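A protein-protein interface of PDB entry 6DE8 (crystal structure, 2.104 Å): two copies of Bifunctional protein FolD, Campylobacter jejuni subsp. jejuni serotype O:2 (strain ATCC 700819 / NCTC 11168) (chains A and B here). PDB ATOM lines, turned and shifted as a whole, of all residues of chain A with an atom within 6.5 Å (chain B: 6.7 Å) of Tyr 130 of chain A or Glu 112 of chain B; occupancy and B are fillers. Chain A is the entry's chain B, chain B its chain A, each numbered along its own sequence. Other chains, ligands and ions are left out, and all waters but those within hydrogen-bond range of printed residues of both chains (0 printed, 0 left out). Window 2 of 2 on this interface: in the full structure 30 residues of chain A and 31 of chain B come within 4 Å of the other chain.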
ATOM      1  N   SER A 116       6.174 -10.162  -6.723  1.00  0.00           N
ATOM      2  CA  SER A 116       5.595 -11.350  -6.106  1.00  0.00           C
ATOM      3  C   SER A 116       6.015 -11.510  -4.652  1.00  0.00           C
ATOM      4  O   SER A 116       5.298 -12.155  -3.881  1.00  0.00           O
ATOM      5  CB  SER A 116       5.979 -12.602  -6.899  1.00  0.00           C
ATOM      6  OG  SER A 116       7.357 -12.896  -6.756  1.00  0.00           O
ATOM      7  N   PRO A 125       0.328 -14.275 -10.706  1.00  0.00           N
ATOM      8  CA  PRO A 125       0.268 -15.597 -11.357  1.00  0.00           C
ATOM      9  C   PRO A 125       1.246 -16.618 -10.796  1.00  0.00           C
ATOM     10  O   PRO A 125       0.901 -17.802 -10.701  1.00  0.00           O
ATOM     11  CB  PRO A 125       0.573 -15.265 -12.823  1.00  0.00           C
ATOM     12  CG  PRO A 125       0.082 -13.869 -12.990  1.00  0.00           C
ATOM     13  CD  PRO A 125       0.369 -13.177 -11.688  1.00  0.00           C
ATOM     14  N   ILE A 126       2.455 -16.201 -10.410  1.00  0.00           N
ATOM     15  CA  ILE A 126       3.419 -17.182  -9.923  1.00  0.00           C
ATOM     16  C   ILE A 126       3.040 -17.668  -8.529  1.00  0.00           C
ATOM     17  O   ILE A 126       3.329 -18.814  -8.165  1.00  0.00           O
ATOM     18  CB  ILE A 126       4.850 -16.610  -9.965  1.00  0.00           C
ATOM     19  CG1 ILE A 126       5.873 -17.747  -9.904  1.00  0.00           C
ATOM     20  CG2 ILE A 126       5.085 -15.630  -8.826  1.00  0.00           C
ATOM     21  CD1 ILE A 126       7.289 -17.308 -10.201  1.00  0.00           C
ATOM     22  N   ASN A 127       2.378 -16.825  -7.729  1.00  0.00           N
ATOM     23  CA  ASN A 127       1.893 -17.284  -6.432  1.00  0.00           C
ATOM     24  C   ASN A 127       0.685 -18.197  -6.586  1.00  0.00           C
ATOM     25  O   ASN A 127       0.504 -19.124  -5.788  1.00  0.00           O
ATOM     26  CB  ASN A 127       1.556 -16.089  -5.541  1.00  0.00           C
ATOM     27  CG  ASN A 127       2.793 -15.376  -5.033  1.00  0.00           C
ATOM     28  OD1 ASN A 127       3.800 -16.009  -4.714  1.00  0.00           O
ATOM     29  ND2 ASN A 127       2.726 -14.051  -4.957  1.00  0.00           N
ATOM     30  N   VAL A 128      -0.149 -17.950  -7.597  1.00  0.00           N
ATOM     31  CA  VAL A 128      -1.222 -18.886  -7.917  1.00  0.00           C
ATOM     32  C   VAL A 128      -0.639 -20.221  -8.359  1.00  0.00           C
ATOM     33  O   VAL A 128      -1.124 -21.290  -7.970  1.00  0.00           O
ATOM     34  CB  VAL A 128      -2.150 -18.291  -8.994  1.00  0.00           C
ATOM     35  CG1 VAL A 128      -3.279 -19.258  -9.321  1.00  0.00           C
ATOM     36  CG2 VAL A 128      -2.697 -16.944  -8.544  1.00  0.00           C
ATOM     37  N   GLY A 129       0.421 -20.180  -9.170  1.00  0.00           N
ATOM     38  CA  GLY A 129       1.036 -21.415  -9.625  1.00  0.00           C
ATOM     39  C   GLY A 129       1.671 -22.205  -8.498  1.00  0.00           C
ATOM     40  O   GLY A 129       1.528 -23.429  -8.431  1.00  0.00           O
ATOM     41  N   TYR A 130       2.381 -21.517  -7.598  1.00  0.00           N
ATOM     42  CA  TYR A 130       2.995 -22.182  -6.453  1.00  0.00           C
ATOM     43  C   TYR A 130       1.961 -22.964  -5.651  1.00  0.00           C
ATOM     44  O   TYR A 130       2.175 -24.133  -5.309  1.00  0.00           O
ATOM     45  CB  TYR A 130       3.687 -21.151  -5.558  1.00  0.00           C
ATOM     46  CG  TYR A 130       4.992 -20.600  -6.098  1.00  0.00           C
ATOM     47  CD1 TYR A 130       5.840 -21.384  -6.868  1.00  0.00           C
ATOM     48  CD2 TYR A 130       5.377 -19.293  -5.825  1.00  0.00           C
ATOM     49  CE1 TYR A 130       7.035 -20.878  -7.355  1.00  0.00           C
ATOM     50  CE2 TYR A 130       6.565 -18.778  -6.309  1.00  0.00           C
ATOM     51  CZ  TYR A 130       7.390 -19.575  -7.072  1.00  0.00           C
ATOM     52  OH  TYR A 130       8.574 -19.063  -7.553  1.00  0.00           O
ATOM     53  N   LEU A 131       0.828 -22.326  -5.343  1.00  0.00           N
ATOM     54  CA  LEU A 131      -0.226 -23.001  -4.593  1.00  0.00           C
ATOM     55  C   LEU A 131      -0.781 -24.192  -5.365  1.00  0.00           C
ATOM     56  O   LEU A 131      -1.019 -25.260  -4.789  1.00  0.00           O
ATOM     57  CB  LEU A 131      -1.344 -22.013  -4.258  1.00  0.00           C
ATOM     58  CG  LEU A 131      -2.615 -22.610  -3.648  1.00  0.00           C
ATOM     59  CD1 LEU A 131      -2.311 -23.289  -2.320  1.00  0.00           C
ATOM     60  CD2 LEU A 131      -3.683 -21.539  -3.478  1.00  0.00           C
ATOM     61  N   ASN A 132      -0.996 -24.027  -6.671  1.00  0.00           N
ATOM     62  CA  ASN A 132      -1.596 -25.095  -7.459  1.00  0.00           C
ATOM     63  C   ASN A 132      -0.665 -26.291  -7.608  1.00  0.00           C
ATOM     64  O   ASN A 132      -1.140 -27.410  -7.832  1.00  0.00           O
ATOM     65  CB  ASN A 132      -2.005 -24.560  -8.833  1.00  0.00           C
ATOM     66  CG  ASN A 132      -3.026 -25.443  -9.519  1.00  0.00           C
ATOM     67  OD1 ASN A 132      -4.226 -25.334  -9.261  1.00  0.00           O
ATOM     68  ND2 ASN A 132      -2.556 -26.330 -10.390  1.00  0.00           N
ATOM     69  N   LEU A 133       0.647 -26.085  -7.484  1.00  0.00           N
ATOM     70  CA  LEU A 133       1.615 -27.174  -7.502  1.00  0.00           C
ATOM     71  C   LEU A 133       1.745 -27.874  -6.154  1.00  0.00           C
ATOM     72  O   LEU A 133       2.644 -28.706  -5.987  1.00  0.00           O
ATOM     73  CB  LEU A 133       2.988 -26.656  -7.943  1.00  0.00           C
ATOM     74  CG  LEU A 133       3.115 -26.132  -9.373  1.00  0.00           C
ATOM     75  CD1 LEU A 133       4.447 -25.425  -9.570  1.00  0.00           C
ATOM     76  CD2 LEU A 133       2.952 -27.263 -10.376  1.00  0.00           C
ATOM     77  N   GLY A 134       0.876 -27.562  -5.194  1.00  0.00           N
ATOM     78  CA  GLY A 134       0.981 -28.116  -3.862  1.00  0.00           C
ATOM     79  C   GLY A 134       2.020 -27.462  -2.980  1.00  0.00           C
ATOM     80  O   GLY A 134       2.244 -27.935  -1.860  1.00  0.00           O
ATOM     81  N   LEU A 135       2.662 -26.396  -3.450  1.00  0.00           N
ATOM     82  CA  LEU A 135       3.687 -25.688  -2.687  1.00  0.00           C
ATOM     83  C   LEU A 135       3.008 -24.548  -1.939  1.00  0.00           C
ATOM     84  O   LEU A 135       2.731 -23.491  -2.512  1.00  0.00           O
ATOM     85  CB  LEU A 135       4.783 -25.170  -3.611  1.00  0.00           C
ATOM     86  CG  LEU A 135       5.223 -26.091  -4.753  1.00  0.00           C
ATOM     87  CD1 LEU A 135       6.251 -25.397  -5.634  1.00  0.00           C
ATOM     88  CD2 LEU A 135       5.771 -27.404  -4.218  1.00  0.00           C
ATOM     89  N   GLU A 136       2.735 -24.759  -0.653  1.00  0.00           N
ATOM     90  CA  GLU A 136       2.098 -23.747   0.186  1.00  0.00           C
ATOM     91  C   GLU A 136       3.119 -22.925   0.959  1.00  0.00           C
ATOM     92  O   GLU A 136       2.884 -22.540   2.108  1.00  0.00           O
ATOM     93  CB  GLU A 136       1.099 -24.402   1.135  1.00  0.00           C
ATOM     94  CG  GLU A 136       0.144 -25.366   0.442  1.00  0.00           C
ATOM     95  CD  GLU A 136      -1.231 -25.392   1.079  1.00  0.00           C
ATOM     96  OE1 GLU A 136      -2.214 -25.657   0.355  1.00  0.00           O
ATOM     97  OE2 GLU A 136      -1.331 -25.132   2.298  1.00  0.00           O
ATOM     98  N   SER A 137       4.264 -22.640   0.340  1.00  0.00           N
ATOM     99  CA  SER A 137       5.324 -21.869   0.975  1.00  0.00           C
ATOM    100  C   SER A 137       5.209 -20.378   0.688  1.00  0.00           C
ATOM    101  O   SER A 137       5.551 -19.555   1.544  1.00  0.00           O
ATOM    102  CB  SER A 137       6.689 -22.383   0.510  1.00  0.00           C
ATOM    103  OG  SER A 137       6.786 -22.354  -0.904  1.00  0.00           O
ATOM    104  N   GLY A 138       4.729 -20.011  -0.499  1.00  0.00           N
ATOM    105  CA  GLY A 138       4.629 -18.620  -0.899  1.00  0.00           C
ATOM    106  C   GLY A 138       3.432 -17.915  -0.300  1.00  0.00           C
ATOM    107  O   GLY A 138       2.991 -18.213   0.815  1.00  0.00           O
ATOM    108  N   PHE A 139       2.896 -16.959  -1.054  1.00  0.00           N
ATOM    109  CA  PHE A 139       1.761 -16.163  -0.607  1.00  0.00           C
ATOM    110  C   PHE A 139       0.463 -16.828  -1.048  1.00  0.00           C
ATOM    111  O   PHE A 139       0.265 -17.089  -2.241  1.00  0.00           O
ATOM    112  CB  PHE A 139       1.846 -14.739  -1.151  1.00  0.00           C
ATOM    113  CG  PHE A 139       2.838 -13.872  -0.431  1.00  0.00           C
ATOM    114  CD1 PHE A 139       2.631 -13.516   0.891  1.00  0.00           C
ATOM    115  CD2 PHE A 139       3.970 -13.404  -1.077  1.00  0.00           C
ATOM    116  CE1 PHE A 139       3.540 -12.716   1.558  1.00  0.00           C
ATOM    117  CE2 PHE A 139       4.881 -12.601  -0.415  1.00  0.00           C
ATOM    118  CZ  PHE A 139       4.666 -12.258   0.904  1.00  0.00           C
ATOM    119  N   ASN A 182      -5.031 -29.977  -1.637  1.00  0.00           N
ATOM    120  CA  ASN A 182      -3.712 -30.184  -1.049  1.00  0.00           C
ATOM    121  C   ASN A 182      -3.808 -30.856   0.314  1.00  0.00           C
ATOM    122  O   ASN A 182      -2.878 -31.559   0.725  1.00  0.00           O
ATOM    123  CB  ASN A 182      -2.965 -28.854  -0.927  1.00  0.00           C
ATOM    124  CG  ASN A 182      -2.584 -28.272  -2.274  1.00  0.00           C
ATOM    125  OD1 ASN A 182      -2.514 -28.985  -3.275  1.00  0.00           O
ATOM    126  ND2 ASN A 182      -2.326 -26.969  -2.303  1.00  0.00           N
ATOM    127  N   LYS B 107      12.721 -32.108  -9.102  1.00  0.00           N
ATOM    128  CA  LYS B 107      12.014 -31.818 -10.346  1.00  0.00           C
ATOM    129  C   LYS B 107      11.452 -30.401 -10.357  1.00  0.00           C
ATOM    130  O   LYS B 107      11.555 -29.694 -11.368  1.00  0.00           O
ATOM    131  CB  LYS B 107      10.891 -32.833 -10.561  1.00  0.00           C
ATOM    132  CG  LYS B 107      10.104 -32.624 -11.846  1.00  0.00           C
ATOM    133  CD  LYS B 107       8.980 -33.640 -11.992  1.00  0.00           C
ATOM    134  CE  LYS B 107       7.711 -33.188 -11.288  1.00  0.00           C
ATOM    135  NZ  LYS B 107       6.600 -32.976 -12.261  1.00  0.00           N
ATOM    136  N   ASP B 108      10.852 -29.971  -9.244  1.00  0.00           N
ATOM    137  CA  ASP B 108      10.213 -28.659  -9.206  1.00  0.00           C
ATOM    138  C   ASP B 108      11.215 -27.537  -9.453  1.00  0.00           C
ATOM    139  O   ASP B 108      10.934 -26.601 -10.210  1.00  0.00           O
ATOM    140  CB  ASP B 108       9.499 -28.467  -7.868  1.00  0.00           C
ATOM    141  CG  ASP B 108       8.189 -29.231  -7.790  1.00  0.00           C
ATOM    142  OD1 ASP B 108       7.455 -29.259  -8.802  1.00  0.00           O
ATOM    143  OD2 ASP B 108       7.894 -29.809  -6.722  1.00  0.00           O
ATOM    144  N   LEU B 109      12.389 -27.611  -8.825  1.00  0.00           N
ATOM    145  CA  LEU B 109      13.396 -26.576  -9.027  1.00  0.00           C
ATOM    146  C   LEU B 109      13.920 -26.577 -10.456  1.00  0.00           C
ATOM    147  O   LEU B 109      14.232 -25.511 -11.001  1.00  0.00           O
ATOM    148  CB  LEU B 109      14.539 -26.761  -8.031  1.00  0.00           C
ATOM    149  CG  LEU B 109      15.625 -25.686  -8.016  1.00  0.00           C
ATOM    150  CD1 LEU B 109      14.994 -24.303  -7.929  1.00  0.00           C
ATOM    151  CD2 LEU B 109      16.600 -25.939  -6.860  1.00  0.00           C
ATOM    152  N   ILE B 110      14.021 -27.758 -11.074  1.00  0.00           N
ATOM    153  CA  ILE B 110      14.482 -27.840 -12.457  1.00  0.00           C
ATOM    154  C   ILE B 110      13.458 -27.226 -13.406  1.00  0.00           C
ATOM    155  O   ILE B 110      13.810 -26.452 -14.306  1.00  0.00           O
ATOM    156  CB  ILE B 110      14.791 -29.302 -12.826  1.00  0.00           C
ATOM    157  CG1 ILE B 110      15.995 -29.809 -12.033  1.00  0.00           C
ATOM    158  CG2 ILE B 110      15.036 -29.441 -14.319  1.00  0.00           C
ATOM    159  CD1 ILE B 110      17.263 -29.025 -12.272  1.00  0.00           C
ATOM    160  N   LEU B 111      12.177 -27.544 -13.214  1.00  0.00           N
ATOM    161  CA  LEU B 111      11.155 -27.061 -14.138  1.00  0.00           C
ATOM    162  C   LEU B 111      10.949 -25.556 -14.024  1.00  0.00           C
ATOM    163  O   LEU B 111      10.601 -24.907 -15.016  1.00  0.00           O
ATOM    164  CB  LEU B 111       9.840 -27.805 -13.900  1.00  0.00           C
ATOM    165  CG  LEU B 111       9.879 -29.294 -14.255  1.00  0.00           C
ATOM    166  CD1 LEU B 111       8.541 -29.962 -13.976  1.00  0.00           C
ATOM    167  CD2 LEU B 111      10.285 -29.488 -15.707  1.00  0.00           C
ATOM    168  N   GLU B 112      11.164 -24.981 -12.838  1.00  0.00           N
ATOM    169  CA  GLU B 112      11.000 -23.540 -12.680  1.00  0.00           C
ATOM    170  C   GLU B 112      12.140 -22.755 -13.319  1.00  0.00           C
ATOM    171  O   GLU B 112      11.961 -21.574 -13.635  1.00  0.00           O
ATOM    172  CB  GLU B 112      10.875 -23.181 -11.195  1.00  0.00           C
ATOM    173  CG  GLU B 112      10.475 -21.732 -10.935  1.00  0.00           C
ATOM    174  CD  GLU B 112      10.258 -21.432  -9.462  1.00  0.00           C
ATOM    175  OE1 GLU B 112      10.368 -22.363  -8.636  1.00  0.00           O
ATOM    176  OE2 GLU B 112       9.975 -20.260  -9.131  1.00  0.00           O
ATOM    177  N   SER B 113      13.301 -23.381 -13.529  1.00  0.00           N
ATOM    178  CA  SER B 113      14.423 -22.686 -14.148  1.00  0.00           C
ATOM    179  C   SER B 113      14.269 -22.548 -15.657  1.00  0.00           C
ATOM    180  O   SER B 113      14.947 -21.711 -16.260  1.00  0.00           O
ATOM    181  CB  SER B 113      15.734 -23.407 -13.838  1.00  0.00           C
ATOM    182  OG  SER B 113      15.837 -24.616 -14.571  1.00  0.00           O
ATOM    183  N   ILE B 114      13.409 -23.355 -16.276  1.00  0.00           N
ATOM    184  CA  ILE B 114      13.110 -23.188 -17.691  1.00  0.00           C
ATOM    185  C   ILE B 114      12.396 -21.859 -17.891  1.00  0.00           C
ATOM    186  O   ILE B 114      11.422 -21.553 -17.191  1.00  0.00           O
ATOM    187  CB  ILE B 114      12.258 -24.359 -18.205  1.00  0.00           C
ATOM    188  CG1 ILE B 114      13.011 -25.682 -18.046  1.00  0.00           C
ATOM    189  CG2 ILE B 114      11.854 -24.131 -19.654  1.00  0.00           C
ATOM    190  CD1 ILE B 114      12.179 -26.899 -18.398  1.00  0.00           C
ATOM    191  N   ILE B 115      12.886 -21.055 -18.837  1.00  0.00           N
ATOM    192  CA  ILE B 115      12.246 -19.775 -19.113  1.00  0.00           C
ATOM    193  C   ILE B 115      10.828 -20.032 -19.605  1.00  0.00           C
ATOM    194  O   ILE B 115      10.584 -20.938 -20.414  1.00  0.00           O
ATOM    195  CB  ILE B 115      13.082 -18.955 -20.111  1.00  0.00           C
ATOM    196  CG1 ILE B 115      12.567 -17.517 -20.196  1.00  0.00           C
ATOM    197  CG2 ILE B 115      13.102 -19.603 -21.492  1.00  0.00           C
ATOM    198  CD1 ILE B 115      13.476 -16.593 -20.984  1.00  0.00           C
ATOM    199  N   SER B 116       9.875 -19.256 -19.085  1.00  0.00           N
ATOM    200  CA  SER B 116       8.467 -19.565 -19.303  1.00  0.00           C
ATOM    201  C   SER B 116       8.041 -19.396 -20.756  1.00  0.00           C
ATOM    202  O   SER B 116       7.035 -19.985 -21.162  1.00  0.00           O
ATOM    203  CB  SER B 116       7.589 -18.697 -18.398  1.00  0.00           C
ATOM    204  OG  SER B 116       7.755 -17.323 -18.690  1.00  0.00           O
ATOM    205  N   PHE B 123       4.700 -26.451 -17.330  1.00  0.00           N
ATOM    206  CA  PHE B 123       4.903 -26.804 -15.933  1.00  0.00           C
ATOM    207  C   PHE B 123       5.466 -25.666 -15.092  1.00  0.00           C
ATOM    208  O   PHE B 123       5.455 -25.770 -13.861  1.00  0.00           O
ATOM    209  CB  PHE B 123       5.829 -28.023 -15.823  1.00  0.00           C
ATOM    210  CG  PHE B 123       5.232 -29.289 -16.369  1.00  0.00           C
ATOM    211  CD1 PHE B 123       3.856 -29.454 -16.422  1.00  0.00           C
ATOM    212  CD2 PHE B 123       6.042 -30.313 -16.828  1.00  0.00           C
ATOM    213  CE1 PHE B 123       3.301 -30.614 -16.925  1.00  0.00           C
ATOM    214  CE2 PHE B 123       5.492 -31.479 -17.333  1.00  0.00           C
ATOM    215  CZ  PHE B 123       4.120 -31.629 -17.381  1.00  0.00           C
ATOM    216  N   HIS B 124       5.952 -24.593 -15.713  1.00  0.00           N
ATOM    217  CA  HIS B 124       6.482 -23.476 -14.944  1.00  0.00           C
ATOM    218  C   HIS B 124       5.381 -22.883 -14.067  1.00  0.00           C
ATOM    219  O   HIS B 124       4.224 -22.800 -14.497  1.00  0.00           O
ATOM    220  CB  HIS B 124       7.058 -22.402 -15.870  1.00  0.00           C
ATOM    221  CG  HIS B 124       7.821 -21.329 -15.155  1.00  0.00           C
ATOM    222  ND1 HIS B 124       7.206 -20.355 -14.399  1.00  0.00           N
ATOM    223  CD2 HIS B 124       9.150 -21.076 -15.083  1.00  0.00           C
ATOM    224  CE1 HIS B 124       8.121 -19.551 -13.889  1.00  0.00           C
ATOM    225  NE2 HIS B 124       9.310 -19.966 -14.289  1.00  0.00           N
ATOM    226  N   PRO B 125       5.699 -22.482 -12.832  1.00  0.00           N
ATOM    227  CA  PRO B 125       4.657 -21.943 -11.939  1.00  0.00           C
ATOM    228  C   PRO B 125       3.841 -20.804 -12.530  1.00  0.00           C
ATOM    229  O   PRO B 125       2.629 -20.737 -12.291  1.00  0.00           O
ATOM    230  CB  PRO B 125       5.468 -21.487 -10.719  1.00  0.00           C
ATOM    231  CG  PRO B 125       6.625 -22.423 -10.685  1.00  0.00           C
ATOM    232  CD  PRO B 125       6.978 -22.688 -12.128  1.00  0.00           C
ATOM    233  N   ILE B 126       4.458 -19.908 -13.304  1.00  0.00           N
ATOM    234  CA  ILE B 126       3.693 -18.787 -13.841  1.00  0.00           C
ATOM    235  C   ILE B 126       2.749 -19.253 -14.944  1.00  0.00           C
ATOM    236  O   ILE B 126       1.688 -18.651 -15.154  1.00  0.00           O
ATOM    237  CB  ILE B 126       4.632 -17.667 -14.325  1.00  0.00           C
ATOM    238  CG1 ILE B 126       3.881 -16.334 -14.355  1.00  0.00           C
ATOM    239  CG2 ILE B 126       5.197 -17.985 -15.704  1.00  0.00           C
ATOM    240  CD1 ILE B 126       4.786 -15.126 -14.442  1.00  0.00           C
ATOM    241  N   VAL B 128       1.364 -22.343 -14.872  1.00  0.00           N
ATOM    242  CA  VAL B 128       0.313 -22.947 -14.059  1.00  0.00           C
ATOM    243  C   VAL B 128      -0.615 -21.870 -13.517  1.00  0.00           C
ATOM    244  O   VAL B 128      -1.836 -22.057 -13.443  1.00  0.00           O
ATOM    245  CB  VAL B 128       0.932 -23.785 -12.921  1.00  0.00           C
ATOM    246  CG1 VAL B 128      -0.155 -24.353 -12.019  1.00  0.00           C
ATOM    247  CG2 VAL B 128       1.801 -24.899 -13.488  1.00  0.00           C
ATOM    248  N   GLY B 129      -0.051 -20.722 -13.137  1.00  0.00           N
ATOM    249  CA  GLY B 129      -0.873 -19.640 -12.618  1.00  0.00           C
ATOM    250  C   GLY B 129      -1.763 -19.015 -13.676  1.00  0.00           C
ATOM    251  O   GLY B 129      -2.930 -18.710 -13.414  1.00  0.00           O
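Of the printed residues of chain B, Pro 125 of chain A touches Pro 125 (3.8 Å), Ile 126 (3.8 Å) and Gly 129 (3.2 Å).
Of the printed residues of chain B, Ile 126 of chain A touches Pro 125.
Tyr 130 of chain A touches two residues of chain B.
Of the printed residues of chain B, Asn 132 of chain A touches Val 128.
Glu 112 of chain B touches one residue of chain A.
Of the printed residues of chain A, Ile 126 of chain B touches Pro 125.
The nearest residue of chain B that does not touch Tyr 130 of chain A is Val 128 of chain B (5.8 Å).
The nearest residue of chain A that does not touch Glu 112 of chain B is Ile 126 of chain A (4.1 Å).
Pro 125 of chain A touches its own counterpart, Pro 125 of chain B.
Pro 125 of chain A touches Gly 129 of chain B, and with the chains exchanged Gly 129 of chain A touches Pro 125 of chain B.
Gly 129 of chain A touches Val 128 of chain B, but with the chains exchanged Val 128 of chain A does not touch Gly 129 of chain B (4.1 Å).
Gly 129 of chain B touches its own counterpart, Gly 129 of chain A.
Of the 11 pairs that touch across the chains among the printed residues, 6 have their exchanged pair printed and touching as well.
A ring nitrogen (ND1) of His 124 of chain B is in hydrogen-bond range of the backbone NH of Ile 126 of chain B (3.0 Å).
NE2 of His 124 of chain B lies within hydrogen-bond range of O of Glu 112 of chain B (3.2 Å).
The backbone carbonyl oxygen (O) of Tyr 130 of chain A sits at hydrogen-bond distance from the backbone NH (N) of Leu 135 of chain A, 3.0 Å away.
The side-chain hydroxyl of Tyr 130 of chain A is in hydrogen-bond range of the side-chain carboxylate of Glu 112 of chain B, at 2.4 Å.
Printed residues of chain A that touch a printed residue of chain B: Pro 125, Ile 126, Gly 129, Tyr 130, Asn 132 and Leu 133.
Hydrophobic or aromatic side chains of chain A within 4 Å of the printed part of chain B: Pro 125, Ile 126, Tyr 130 and Leu 133.
Among the printed residues, no Asp or Glu carboxylate lies within 4 Å of a Lys or Arg side-chain nitrogen of the other chain.
Among the printed residues, merely in contact across the chains: Pro 125 of chain A with Pro 125 of chain B, Pro 125 of chain A with Ile 126 of chain B, Pro 125 of chain A with Gly 129 of chain B, Ile 126 of chain A with Pro 125 of chain B, Gly 129 of chain A with Pro 125 of chain B, Gly 129 of chain A with Val 128 of chain B, Gly 129 of chain A with Gly 129 of chain B, Tyr 130 of chain A with Pro 125 of chain B, Asn 132 of chain A with Val 128 of chain B and Leu 133 of chain A with Pro 125 of chain B.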
